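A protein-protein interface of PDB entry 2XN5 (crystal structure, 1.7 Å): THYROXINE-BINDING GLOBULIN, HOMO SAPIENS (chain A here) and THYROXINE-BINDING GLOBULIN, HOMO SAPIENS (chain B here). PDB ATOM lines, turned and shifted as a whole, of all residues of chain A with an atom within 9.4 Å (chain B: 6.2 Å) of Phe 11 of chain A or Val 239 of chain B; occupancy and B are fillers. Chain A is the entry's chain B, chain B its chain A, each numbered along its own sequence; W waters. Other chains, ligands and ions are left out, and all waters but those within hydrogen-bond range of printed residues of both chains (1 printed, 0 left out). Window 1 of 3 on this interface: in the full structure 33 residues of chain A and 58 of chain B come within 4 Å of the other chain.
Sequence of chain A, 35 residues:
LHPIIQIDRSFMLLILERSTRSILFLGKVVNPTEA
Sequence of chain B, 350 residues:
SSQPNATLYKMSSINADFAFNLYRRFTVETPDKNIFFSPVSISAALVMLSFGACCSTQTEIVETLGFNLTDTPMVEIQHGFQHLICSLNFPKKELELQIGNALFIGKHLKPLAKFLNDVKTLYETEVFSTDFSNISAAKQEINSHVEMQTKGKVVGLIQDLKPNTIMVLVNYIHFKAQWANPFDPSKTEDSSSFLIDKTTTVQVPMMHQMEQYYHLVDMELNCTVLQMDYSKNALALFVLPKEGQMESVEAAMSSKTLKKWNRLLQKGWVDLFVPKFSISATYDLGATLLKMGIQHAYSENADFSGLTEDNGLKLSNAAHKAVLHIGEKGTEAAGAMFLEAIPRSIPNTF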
ATOM      1  N   ILE A   5      21.173 -11.678  14.861  1.00  0.00           N
ATOM      2  CA  ILE A   5      22.002 -11.168  13.775  1.00  0.00           C
ATOM      3  C   ILE A   5      23.400 -10.951  14.326  1.00  0.00           C
ATOM      4  O   ILE A   5      23.591 -10.154  15.239  1.00  0.00           O
ATOM      5  CB  ILE A   5      21.457  -9.869  13.158  1.00  0.00           C
ATOM      6  CG1 ILE A   5      20.090 -10.123  12.501  1.00  0.00           C
ATOM      7  CG2 ILE A   5      22.455  -9.327  12.129  1.00  0.00           C
ATOM      8  CD1 ILE A   5      19.439  -8.866  11.879  1.00  0.00           C
ATOM      9  N   GLN A   6      24.356 -11.708  13.784  1.00  0.00           N
ATOM     10  CA  GLN A   6      25.747 -11.655  14.226  1.00  0.00           C
ATOM     11  C   GLN A   6      26.615 -11.121  13.103  1.00  0.00           C
ATOM     12  O   GLN A   6      26.834 -11.804  12.102  1.00  0.00           O
ATOM     13  CB  GLN A   6      26.240 -13.053  14.617  1.00  0.00           C
ATOM     14  CG  GLN A   6      26.003 -13.422  16.055  1.00  0.00           C
ATOM     15  CD  GLN A   6      26.480 -14.824  16.376  1.00  0.00           C
ATOM     16  OE1 GLN A   6      25.988 -15.799  15.816  1.00  0.00           O
ATOM     17  NE2 GLN A   6      27.434 -14.929  17.296  1.00  0.00           N
ATOM     18  N   ILE A   7      27.125  -9.906  13.281  1.00  0.00           N
ATOM     19  CA  ILE A   7      27.997  -9.292  12.290  1.00  0.00           C
ATOM     20  C   ILE A   7      29.422  -9.785  12.563  1.00  0.00           C
ATOM     21  O   ILE A   7      30.235  -9.068  13.145  1.00  0.00           O
ATOM     22  CB  ILE A   7      27.910  -7.747  12.328  1.00  0.00           C
ATOM     23  CG1 ILE A   7      26.456  -7.282  12.227  1.00  0.00           C
ATOM     24  CG2 ILE A   7      28.724  -7.147  11.194  1.00  0.00           C
ATOM     25  CD1 ILE A   7      25.710  -7.875  11.082  1.00  0.00           C
ATOM     26  N   ASP A   8      29.694 -11.028  12.156  1.00  0.00           N
ATOM     27  CA  ASP A   8      30.935 -11.732  12.493  1.00  0.00           C
ATOM     28  C   ASP A   8      31.690 -12.218  11.244  1.00  0.00           C
ATOM     29  O   ASP A   8      32.513 -13.132  11.313  1.00  0.00           O
ATOM     30  CB  ASP A   8      30.636 -12.902  13.446  1.00  0.00           C
ATOM     31  CG  ASP A   8      29.768 -13.979  12.807  1.00  0.00           C
ATOM     32  OD1 ASP A   8      29.264 -13.760  11.686  1.00  0.00           O
ATOM     33  OD2 ASP A   8      29.604 -15.053  13.424  1.00  0.00           O
ATOM     34  N   ARG A   9      31.392 -11.600  10.106  1.00  0.00           N
ATOM     35  CA  ARG A   9      32.142 -11.813   8.884  1.00  0.00           C
ATOM     36  C   ARG A   9      31.952 -10.600   7.971  1.00  0.00           C
ATOM     37  O   ARG A   9      31.214  -9.669   8.314  1.00  0.00           O
ATOM     38  CB  ARG A   9      31.714 -13.119   8.190  1.00  0.00           C
ATOM     39  CG  ARG A   9      30.243 -13.196   7.826  1.00  0.00           C
ATOM     40  CD  ARG A   9      29.928 -14.399   6.950  1.00  0.00           C
ATOM     41  NE  ARG A   9      28.563 -14.350   6.411  1.00  0.00           N
ATOM     42  CZ  ARG A   9      27.455 -14.607   7.105  1.00  0.00           C
ATOM     43  NH1 ARG A   9      27.504 -14.941   8.386  1.00  0.00           N
ATOM     44  NH2 ARG A   9      26.276 -14.532   6.508  1.00  0.00           N
ATOM     45  N   SER A  10      32.619 -10.612   6.824  1.00  0.00           N
ATOM     46  CA  SER A  10      32.633  -9.466   5.906  1.00  0.00           C
ATOM     47  C   SER A  10      31.242  -8.868   5.725  1.00  0.00           C
ATOM     48  O   SER A  10      30.281  -9.601   5.506  1.00  0.00           O
ATOM     49  CB  SER A  10      33.175  -9.871   4.529  1.00  0.00           C
ATOM     50  OG  SER A  10      34.571 -10.069   4.554  1.00  0.00           O
ATOM     51  N   PHE A  11      31.157  -7.541   5.816  1.00  0.00           N
ATOM     52  CA  PHE A  11      29.909  -6.821   5.627  1.00  0.00           C
ATOM     53  C   PHE A  11      30.111  -5.480   4.924  1.00  0.00           C
ATOM     54  O   PHE A  11      31.182  -4.896   5.002  1.00  0.00           O
ATOM     55  CB  PHE A  11      29.206  -6.596   6.980  1.00  0.00           C
ATOM     56  CG  PHE A  11      29.962  -5.728   7.953  1.00  0.00           C
ATOM     57  CD1 PHE A  11      30.848  -6.292   8.857  1.00  0.00           C
ATOM     58  CD2 PHE A  11      29.716  -4.359   8.031  1.00  0.00           C
ATOM     59  CE1 PHE A  11      31.524  -5.509   9.785  1.00  0.00           C
ATOM     60  CE2 PHE A  11      30.389  -3.566   8.946  1.00  0.00           C
ATOM     61  CZ  PHE A  11      31.298  -4.141   9.835  1.00  0.00           C
ATOM     62  N   MET A  12      29.090  -5.017   4.211  1.00  0.00           N
ATOM     63  CA  MET A  12      29.073  -3.636   3.710  1.00  0.00           C
ATOM     64  C   MET A  12      28.409  -2.724   4.739  1.00  0.00           C
ATOM     65  O   MET A  12      27.513  -3.145   5.488  1.00  0.00           O
ATOM     66  CB  MET A  12      28.360  -3.545   2.347  1.00  0.00           C
ATOM     67  CG  MET A  12      29.164  -4.102   1.170  1.00  0.00           C
ATOM     68  SD  MET A  12      28.333  -3.886  -0.435  1.00  0.00           S
ATOM     69  CE  MET A  12      28.362  -2.108  -0.630  1.00  0.00           C
ATOM     70  N   LEU A  13      28.848  -1.469   4.763  1.00  0.00           N
ATOM     71  CA  LEU A  13      28.373  -0.458   5.698  1.00  0.00           C
ATOM     72  C   LEU A  13      28.041   0.803   4.916  1.00  0.00           C
ATOM     73  O   LEU A  13      28.810   1.213   4.028  1.00  0.00           O
ATOM     74  CB  LEU A  13      29.477  -0.110   6.690  1.00  0.00           C
ATOM     75  CG  LEU A  13      29.187   0.965   7.741  1.00  0.00           C
ATOM     76  CD1 LEU A  13      28.098   0.498   8.707  1.00  0.00           C
ATOM     77  CD2 LEU A  13      30.443   1.322   8.504  1.00  0.00           C
ATOM     78  N   LEU A  14      26.906   1.410   5.247  1.00  0.00           N
ATOM     79  CA  LEU A  14      26.521   2.694   4.688  1.00  0.00           C
ATOM     80  C   LEU A  14      26.077   3.609   5.807  1.00  0.00           C
ATOM     81  O   LEU A  14      25.367   3.181   6.712  1.00  0.00           O
ATOM     82  CB  LEU A  14      25.361   2.526   3.690  1.00  0.00           C
ATOM     83  CG  LEU A  14      25.557   1.599   2.490  1.00  0.00           C
ATOM     84  CD1 LEU A  14      25.310   0.130   2.832  1.00  0.00           C
ATOM     85  CD2 LEU A  14      24.640   2.061   1.367  1.00  0.00           C
ATOM     86  N   ILE A  15      26.485   4.868   5.753  1.00  0.00           N
ATOM     87  CA  ILE A  15      25.960   5.870   6.669  1.00  0.00           C
ATOM     88  C   ILE A  15      25.182   6.872   5.825  1.00  0.00           C
ATOM     89  O   ILE A  15      25.720   7.433   4.866  1.00  0.00           O
ATOM     90  CB  ILE A  15      27.088   6.555   7.453  1.00  0.00           C
ATOM     91  CG1 ILE A  15      27.804   5.534   8.349  1.00  0.00           C
ATOM     92  CG2 ILE A  15      26.534   7.711   8.298  1.00  0.00           C
ATOM     93  CD1 ILE A  15      29.031   6.114   9.054  1.00  0.00           C
ATOM     94  N   LEU A  26      30.465   5.049   2.695  1.00  0.00           N
ATOM     95  CA  LEU A  26      30.201   3.731   2.121  1.00  0.00           C
ATOM     96  C   LEU A  26      31.450   2.907   2.282  1.00  0.00           C
ATOM     97  O   LEU A  26      32.566   3.406   2.079  1.00  0.00           O
ATOM     98  CB  LEU A  26      29.856   3.857   0.623  1.00  0.00           C
ATOM     99  CG  LEU A  26      29.630   2.581  -0.200  1.00  0.00           C
ATOM    100  CD1 LEU A  26      28.487   1.727   0.359  1.00  0.00           C
ATOM    101  CD2 LEU A  26      29.356   2.915  -1.690  1.00  0.00           C
ATOM    102  N   GLY A  27      31.290   1.628   2.618  1.00  0.00           N
ATOM    103  CA  GLY A  27      32.455   0.803   2.761  1.00  0.00           C
ATOM    104  C   GLY A  27      32.159  -0.667   2.872  1.00  0.00           C
ATOM    105  O   GLY A  27      31.002  -1.072   2.907  1.00  0.00           O
ATOM    106  N   LYS A  28      33.234  -1.444   2.878  1.00  0.00           N
ATOM    107  CA  LYS A  28      33.185  -2.868   3.190  1.00  0.00           C
ATOM    108  C   LYS A  28      34.242  -3.177   4.223  1.00  0.00           C
ATOM    109  O   LYS A  28      35.405  -2.779   4.064  1.00  0.00           O
ATOM    110  CB  LYS A  28      33.448  -3.705   1.957  1.00  0.00           C
ATOM    111  CG  LYS A  28      33.586  -5.193   2.236  1.00  0.00           C
ATOM    112  CD  LYS A  28      33.611  -6.020   0.958  1.00  0.00           C
ATOM    113  CE  LYS A  28      34.755  -5.626   0.032  1.00  0.00           C
ATOM    114  NZ  LYS A  28      34.985  -6.619  -1.060  1.00  0.00           N
ATOM    115  N   VAL A  29      33.838  -3.893   5.265  1.00  0.00           N
ATOM    116  CA  VAL A  29      34.749  -4.307   6.326  1.00  0.00           C
ATOM    117  C   VAL A  29      35.048  -5.789   6.128  1.00  0.00           C
ATOM    118  O   VAL A  29      34.174  -6.617   6.334  1.00  0.00           O
ATOM    119  CB  VAL A  29      34.126  -4.044   7.700  1.00  0.00           C
ATOM    120  CG1 VAL A  29      35.026  -4.554   8.810  1.00  0.00           C
ATOM    121  CG2 VAL A  29      33.885  -2.532   7.859  1.00  0.00           C
ATOM    122  N   VAL A  30      36.269  -6.095   5.689  1.00  0.00           N
ATOM    123  CA  VAL A  30      36.740  -7.479   5.524  1.00  0.00           C
ATOM    124  C   VAL A  30      37.531  -7.935   6.754  1.00  0.00           C
ATOM    125  O   VAL A  30      37.369  -9.055   7.224  1.00  0.00           O
ATOM    126  CB  VAL A  30      37.619  -7.627   4.262  1.00  0.00           C
ATOM    127  CG1 VAL A  30      38.107  -9.068   4.093  1.00  0.00           C
ATOM    128  CG2 VAL A  30      36.872  -7.169   3.019  1.00  0.00           C
ATOM    129  N   ASN A  31      38.395  -7.061   7.256  1.00  0.00           N
ATOM    130  CA  ASN A  31      39.182  -7.321   8.465  1.00  0.00           C
ATOM    131  C   ASN A  31      39.149  -6.080   9.354  1.00  0.00           C
ATOM    132  O   ASN A  31      39.878  -5.116   9.105  1.00  0.00           O
ATOM    133  CB  ASN A  31      40.622  -7.667   8.100  1.00  0.00           C
ATOM    134  CG  ASN A  31      41.495  -7.945   9.330  1.00  0.00           C
ATOM    135  OD1 ASN A  31      41.060  -7.784  10.469  1.00  0.00           O
ATOM    136  ND2 ASN A  31      42.723  -8.370   9.095  1.00  0.00           N
ATOM    137  N   PRO A  32      38.319  -6.106  10.410  1.00  0.00           N
ATOM    138  CA  PRO A  32      38.176  -4.905  11.235  1.00  0.00           C
ATOM    139  C   PRO A  32      39.411  -4.564  12.085  1.00  0.00           C
ATOM    140  O   PRO A  32      39.450  -3.487  12.671  1.00  0.00           O
ATOM    141  CB  PRO A  32      36.946  -5.209  12.109  1.00  0.00           C
ATOM    142  CG  PRO A  32      36.801  -6.678  12.093  1.00  0.00           C
ATOM    143  CD  PRO A  32      37.423  -7.195  10.841  1.00  0.00           C
ATOM    144  N   THR A  33      40.415  -5.443  12.115  1.00  0.00           N
ATOM    145  CA  THR A  33      41.640  -5.208  12.898  1.00  0.00           C
ATOM    146  C   THR A  33      42.850  -4.768  12.055  1.00  0.00           C
ATOM    147  O   THR A  33      43.967  -4.698  12.570  1.00  0.00           O
ATOM    148  CB  THR A  33      42.034  -6.468  13.715  1.00  0.00           C
ATOM    149  OG1 THR A  33      42.502  -7.496  12.835  1.00  0.00           O
ATOM    150  CG2 THR A  33      40.854  -6.994  14.515  1.00  0.00           C
ATOM    151  N   PHE B 194      35.961 -13.058  14.365  1.00  0.00           N
ATOM    152  CA  PHE B 194      35.418 -12.410  13.167  1.00  0.00           C
ATOM    153  C   PHE B 194      36.096 -13.061  11.974  1.00  0.00           C
ATOM    154  O   PHE B 194      37.323 -13.089  11.900  1.00  0.00           O
ATOM    155  CB  PHE B 194      35.684 -10.901  13.192  1.00  0.00           C
ATOM    156  CG  PHE B 194      35.012 -10.134  12.068  1.00  0.00           C
ATOM    157  CD1 PHE B 194      33.847  -9.413  12.296  1.00  0.00           C
ATOM    158  CD2 PHE B 194      35.558 -10.124  10.795  1.00  0.00           C
ATOM    159  CE1 PHE B 194      33.227  -8.706  11.263  1.00  0.00           C
ATOM    160  CE2 PHE B 194      34.946  -9.419   9.758  1.00  0.00           C
ATOM    161  CZ  PHE B 194      33.784  -8.703   9.999  1.00  0.00           C
ATOM    162  N   CYS B 223      20.895 -11.360   1.347  1.00  0.00           N
ATOM    163  CA  CYS B 223      21.654 -10.628   2.347  1.00  0.00           C
ATOM    164  C   CYS B 223      20.720 -10.153   3.451  1.00  0.00           C
ATOM    165  O   CYS B 223      19.543  -9.899   3.212  1.00  0.00           O
ATOM    166  CB  CYS B 223      22.405  -9.427   1.735  1.00  0.00           C
ATOM    167  SG  CYS B 223      21.379  -8.169   0.915  1.00  0.00           S
ATOM    168  N   THR B 224      21.269 -10.057   4.658  1.00  0.00           N
ATOM    169  CA  THR B 224      20.572  -9.505   5.797  1.00  0.00           C
ATOM    170  C   THR B 224      20.921  -8.022   5.844  1.00  0.00           C
ATOM    171  O   THR B 224      22.082  -7.647   5.666  1.00  0.00           O
ATOM    172  CB  THR B 224      21.029 -10.205   7.097  1.00  0.00           C
ATOM    173  OG1 THR B 224      20.629 -11.581   7.065  1.00  0.00           O
ATOM    174  CG2 THR B 224      20.423  -9.550   8.305  1.00  0.00           C
ATOM    175  N   VAL B 225      19.920  -7.182   6.084  1.00  0.00           N
ATOM    176  CA  VAL B 225      20.128  -5.734   6.225  1.00  0.00           C
ATOM    177  C   VAL B 225      19.682  -5.325   7.628  1.00  0.00           C
ATOM    178  O   VAL B 225      18.559  -5.621   8.035  1.00  0.00           O
ATOM    179  CB  VAL B 225      19.361  -4.932   5.148  1.00  0.00           C
ATOM    180  CG1 VAL B 225      19.558  -3.413   5.333  1.00  0.00           C
ATOM    181  CG2 VAL B 225      19.792  -5.353   3.747  1.00  0.00           C
ATOM    182  N   LEU B 226      20.576  -4.670   8.375  1.00  0.00           N
ATOM    183  CA  LEU B 226      20.267  -4.208   9.718  1.00  0.00           C
ATOM    184  C   LEU B 226      20.542  -2.721   9.789  1.00  0.00           C
ATOM    185  O   LEU B 226      21.643  -2.268   9.458  1.00  0.00           O
ATOM    186  CB  LEU B 226      21.113  -4.922  10.774  1.00  0.00           C
ATOM    187  CG  LEU B 226      20.932  -4.294  12.168  1.00  0.00           C
ATOM    188  CD1 LEU B 226      19.855  -5.029  12.936  1.00  0.00           C
ATOM    189  CD2 LEU B 226      22.243  -4.199  12.940  1.00  0.00           C
ATOM    190  N   LEU B 237      23.495   1.502   7.896  1.00  0.00           N
ATOM    191  CA  LEU B 237      23.010   0.215   7.394  1.00  0.00           C
ATOM    192  C   LEU B 237      24.165  -0.763   7.324  1.00  0.00           C
ATOM    193  O   LEU B 237      25.221  -0.464   6.761  1.00  0.00           O
ATOM    194  CB  LEU B 237      22.375   0.348   6.000  1.00  0.00           C
ATOM    195  CG  LEU B 237      21.150   1.248   5.850  1.00  0.00           C
ATOM    196  CD1 LEU B 237      20.809   1.440   4.377  1.00  0.00           C
ATOM    197  CD2 LEU B 237      19.945   0.689   6.611  1.00  0.00           C
ATOM    198  N   PHE B 238      23.974  -1.939   7.920  1.00  0.00           N
ATOM    199  CA  PHE B 238      24.946  -3.022   7.850  1.00  0.00           C
ATOM    200  C   PHE B 238      24.349  -4.074   6.946  1.00  0.00           C
ATOM    201  O   PHE B 238      23.228  -4.530   7.207  1.00  0.00           O
ATOM    202  CB  PHE B 238      25.173  -3.628   9.227  1.00  0.00           C
ATOM    203  CG  PHE B 238      25.809  -2.687  10.199  1.00  0.00           C
ATOM    204  CD1 PHE B 238      25.067  -1.669  10.786  1.00  0.00           C
ATOM    205  CD2 PHE B 238      27.149  -2.813  10.526  1.00  0.00           C
ATOM    206  CE1 PHE B 238      25.654  -0.782  11.691  1.00  0.00           C
ATOM    207  CE2 PHE B 238      27.744  -1.935  11.410  1.00  0.00           C
ATOM    208  CZ  PHE B 238      26.995  -0.919  11.999  1.00  0.00           C
ATOM    209  N   VAL B 239      25.087  -4.455   5.902  1.00  0.00           N
ATOM    210  CA  VAL B 239      24.633  -5.416   4.896  1.00  0.00           C
ATOM    211  C   VAL B 239      25.495  -6.664   4.982  1.00  0.00           C
ATOM    212  O   VAL B 239      26.685  -6.617   4.683  1.00  0.00           O
ATOM    213  CB  VAL B 239      24.744  -4.815   3.494  1.00  0.00           C
ATOM    214  CG1 VAL B 239      24.244  -5.797   2.427  1.00  0.00           C
ATOM    215  CG2 VAL B 239      23.983  -3.501   3.436  1.00  0.00           C
ATOM    216  N   LEU B 240      24.881  -7.776   5.387  1.00  0.00           N
ATOM    217  CA  LEU B 240      25.585  -9.018   5.635  1.00  0.00           C
ATOM    218  C   LEU B 240      25.133 -10.056   4.610  1.00  0.00           C
ATOM    219  O   LEU B 240      24.059 -10.645   4.757  1.00  0.00           O
ATOM    220  CB  LEU B 240      25.316  -9.501   7.065  1.00  0.00           C
ATOM    221  CG  LEU B 240      26.043 -10.760   7.509  1.00  0.00           C
ATOM    222  CD1 LEU B 240      27.534 -10.454   7.716  1.00  0.00           C
ATOM    223  CD2 LEU B 240      25.431 -11.349   8.781  1.00  0.00           C
ATOM    224  N   PRO B 241      25.939 -10.268   3.555  1.00  0.00           N
ATOM    225  CA  PRO B 241      25.586 -11.279   2.575  1.00  0.00           C
ATOM    226  C   PRO B 241      25.612 -12.665   3.179  1.00  0.00           C
ATOM    227  O   PRO B 241      26.363 -12.923   4.127  1.00  0.00           O
ATOM    228  CB  PRO B 241      26.682 -11.142   1.509  1.00  0.00           C
ATOM    229  CG  PRO B 241      27.254  -9.776   1.712  1.00  0.00           C
ATOM    230  CD  PRO B 241      27.166  -9.543   3.172  1.00  0.00           C
ATOM    231  N   MET B 246      28.874 -12.152  -1.288  1.00  0.00           N
ATOM    232  CA  MET B 246      29.324 -10.751  -1.256  1.00  0.00           C
ATOM    233  C   MET B 246      29.456 -10.180  -2.669  1.00  0.00           C
ATOM    234  O   MET B 246      28.961  -9.104  -2.938  1.00  0.00           O
ATOM    235  CB  MET B 246      30.650 -10.608  -0.504  1.00  0.00           C
ATOM    236  CG  MET B 246      31.221  -9.184  -0.504  1.00  0.00           C
ATOM    237  SD  MET B 246      30.189  -7.950   0.298  1.00  0.00           S
ATOM    238  CE  MET B 246      30.594  -8.242   2.027  1.00  0.00           C
ATOM    239  N   VAL B 249      26.048  -9.356  -4.209  1.00  0.00           N
ATOM    240  CA  VAL B 249      25.483  -8.167  -3.549  1.00  0.00           C
ATOM    241  C   VAL B 249      26.165  -6.869  -4.012  1.00  0.00           C
ATOM    242  O   VAL B 249      25.487  -5.889  -4.330  1.00  0.00           O
ATOM    243  CB  VAL B 249      25.545  -8.277  -2.003  1.00  0.00           C
ATOM    244  CG1 VAL B 249      25.179  -6.950  -1.342  1.00  0.00           C
ATOM    245  CG2 VAL B 249      24.596  -9.352  -1.525  1.00  0.00           C
ATOM    246  N   MET B 253      24.171  -3.499  -5.945  1.00  0.00           N
ATOM    247  CA  MET B 253      23.872  -2.262  -5.210  1.00  0.00           C
ATOM    248  C   MET B 253      23.692  -1.044  -6.139  1.00  0.00           C
ATOM    249  O   MET B 253      24.472  -0.812  -7.075  1.00  0.00           O
ATOM    250  CB  MET B 253      24.927  -1.931  -4.143  1.00  0.00           C
ATOM    251  CG  MET B 253      25.059  -2.947  -3.009  1.00  0.00           C
ATOM    252  SD  MET B 253      23.562  -3.156  -2.023  1.00  0.00           S
ATOM    253  CE  MET B 253      23.474  -1.552  -1.218  1.00  0.00           C
ATOM    254  N   TRP B 261      14.759  -1.033  -0.088  1.00  0.00           N
ATOM    255  CA  TRP B 261      14.941  -1.312   1.341  1.00  0.00           C
ATOM    256  C   TRP B 261      14.183  -0.304   2.220  1.00  0.00           C
ATOM    257  O   TRP B 261      13.679  -0.672   3.291  1.00  0.00           O
ATOM    258  CB  TRP B 261      16.430  -1.371   1.741  1.00  0.00           C
ATOM    259  CG  TRP B 261      17.203  -2.555   1.161  1.00  0.00           C
ATOM    260  CD1 TRP B 261      16.682  -3.679   0.575  1.00  0.00           C
ATOM    261  CD2 TRP B 261      18.629  -2.727   1.143  1.00  0.00           C
ATOM    262  NE1 TRP B 261      17.687  -4.522   0.176  1.00  0.00           N
ATOM    263  CE2 TRP B 261      18.893  -3.971   0.519  1.00  0.00           C
ATOM    264  CE3 TRP B 261      19.704  -1.952   1.578  1.00  0.00           C
ATOM    265  CZ2 TRP B 261      20.191  -4.451   0.323  1.00  0.00           C
ATOM    266  CZ3 TRP B 261      20.997  -2.433   1.379  1.00  0.00           C
ATOM    267  CH2 TRP B 261      21.225  -3.677   0.759  1.00  0.00           C
ATOM    268  N   PRO B 275      30.684  -5.640  15.884  1.00  0.00           N
ATOM    269  CA  PRO B 275      32.041  -5.381  16.354  1.00  0.00           C
ATOM    270  C   PRO B 275      32.295  -3.902  16.652  1.00  0.00           C
ATOM    271  O   PRO B 275      31.682  -3.027  16.034  1.00  0.00           O
ATOM    272  CB  PRO B 275      32.915  -5.865  15.187  1.00  0.00           C
ATOM    273  CG  PRO B 275      32.079  -5.715  14.006  1.00  0.00           C
ATOM    274  CD  PRO B 275      30.668  -5.972  14.450  1.00  0.00           C
ATOM    275  N   PHE B 277      35.297  -1.322  16.350  1.00  0.00           N
ATOM    276  CA  PHE B 277      36.480  -1.304  15.490  1.00  0.00           C
ATOM    277  C   PHE B 277      36.704   0.068  14.868  1.00  0.00           C
ATOM    278  O   PHE B 277      35.823   0.927  14.895  1.00  0.00           O
ATOM    279  CB  PHE B 277      36.338  -2.347  14.368  1.00  0.00           C
ATOM    280  CG  PHE B 277      35.306  -1.981  13.335  1.00  0.00           C
ATOM    281  CD1 PHE B 277      35.688  -1.431  12.125  1.00  0.00           C
ATOM    282  CD2 PHE B 277      33.949  -2.153  13.593  1.00  0.00           C
ATOM    283  CE1 PHE B 277      34.750  -1.071  11.190  1.00  0.00           C
ATOM    284  CE2 PHE B 277      33.004  -1.808  12.669  1.00  0.00           C
ATOM    285  CZ  PHE B 277      33.397  -1.257  11.452  1.00  0.00           C
ATOM    286  N   ILE B 326      33.635   2.873  15.136  1.00  0.00           N
ATOM    287  CA  ILE B 326      32.330   2.438  15.659  1.00  0.00           C
ATOM    288  C   ILE B 326      32.550   1.809  17.026  1.00  0.00           C
ATOM    289  O   ILE B 326      33.373   0.903  17.164  1.00  0.00           O
ATOM    290  CB  ILE B 326      31.649   1.418  14.732  1.00  0.00           C
ATOM    291  CG1 ILE B 326      31.046   2.126  13.512  1.00  0.00           C
ATOM    292  CG2 ILE B 326      30.558   0.648  15.475  1.00  0.00           C
ATOM    293  CD1 ILE B 326      30.478   1.172  12.453  1.00  0.00           C
HETATM  294  O   HOH W   1      23.169 -13.037   6.013  1.00  0.00           O
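The backbone NH (N) of Val 29 of chain A sits at hydrogen-bond distance from the backbone carbonyl oxygen (O) of Phe 11 of chain A (2.9 Å).
N of Ile 326 of chain B is in hydrogen-bond range of O of Phe 277 of chain B, 2.9 Å away.
The side-chain carboxylate of Asp 8 of chain A lies within salt-bridge range of the guanidinium group of Arg 9 of chain A, at 3.9 Å.
Among the printed residues, merely in contact across the chains: Ile 5 of chain A with Thr 224 of chain B (3.8 Å), Gln 6 of chain A with Leu 240 of chain B (3.6 Å), Ile 7 of chain A with Phe 194 of chain B (3.6 Å), Ile 7 of chain A with Pro 275 of chain B (3.4 Å), Asp 8 of chain A with Phe 194 of chain B (3.5 Å), Arg 9 of chain A with Phe 194 of chain B (3.2 Å), Arg 9 of chain A with Leu 240 of chain B (3.8 Å), Ser 10 of chain A with Phe 194 of chain B (3.9 Å), Ser 10 of chain A with Leu 240 of chain B (3.6 Å), Ser 10 of chain A with Pro 241 of chain B (3.9 Å), Ser 10 of chain A with Met 246 of chain B (3.7 Å), Phe 11 of chain A with Phe 194 of chain B (3.9 Å), Phe 11 of chain A with Phe 238 of chain B (3.7 Å), Phe 11 of chain A with Val 239 of chain B (3.4 Å), Phe 11 of chain A with Met 246 of chain B (3.9 Å), Phe 11 of chain A with Phe 277 of chain B (3.9 Å), Met 12 of chain A with Leu 237 of chain B (3.7 Å), Met 12 of chain A with Phe 238 of chain B (3.5 Å), Leu 13 of chain A with Leu 237 of chain B (3.3 Å), Leu 13 of chain A with Phe 238 of chain B (3.7 Å), Leu 13 of chain A with Ile 326 of chain B (3.95 Å), Leu 14 of chain A with Val 239 of chain B (3.9 Å), Lys 28 of chain A with Met 246 of chain B (3.9 Å), Val 29 of chain A with Phe 277 of chain B (3.7 Å), Val 30 of chain A with Phe 194 of chain B (3.5 Å), Pro 32 of chain A with Phe 194 of chain B (3.5 Å) and Pro 32 of chain A with Phe 277 of chain B (3.7 Å).
The backbone NH of Leu 237 of chain B lies within hydrogen-bond range of the backbone carbonyl oxygen of Leu 14 of chain A.
The guanidinium group (NH2) of Arg 9 of chain A is in hydrogen-bond range of the backbone carbonyl oxygen (O) of Pro 241 of chain B, 2.9 Å away.
The backbone NH (N) of Val 239 of chain B is in hydrogen-bond range of the backbone carbonyl oxygen (O) of Met 12 of chain A, 2.8 Å away.
Water W1 lies within hydrogen-bond range of the backbone carbonyl oxygen (O) of Leu 240 of chain B, the side-chain hydroxyl (OG1) of Thr 224 of chain B and the guanidinium group (NH2) of Arg 9 of chain A.
Along chain B the printed residues that touch a printed residue of chain A span positions 194 to 326.
Printed residues of chain A that touch a printed residue of chain B: Ile 5, Gln 6, Ile 7, Asp 8, Arg 9, Ser 10, Phe 11, Met 12, Leu 13, Leu 14, Lys 28, Val 29, Val 30 and Pro 32.
Among the printed residues, no Asp or Glu carboxylate lies within 4 Å of a Lys or Arg side-chain nitrogen of the other chain.
Phe 11 of chain A touches five residues of chain B.
Of chain A, only Phe 11 (3.4 Å), Met 12 (2.8 Å) and Leu 14 (3.9 Å) come within 4 Å of Val 239 of chain B.
Printed residues of chain A within 4 Å of Pro 275 of chain B: Ile 7.
Printed residues of chain A within 4 Å of Thr 224 of chain B: Ile 5 (3.8 Å).
Printed residues of chain B within 4 Å of Ile 7 of chain A: Phe 194 (3.6 Å) and Pro 275 (3.4 Å).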
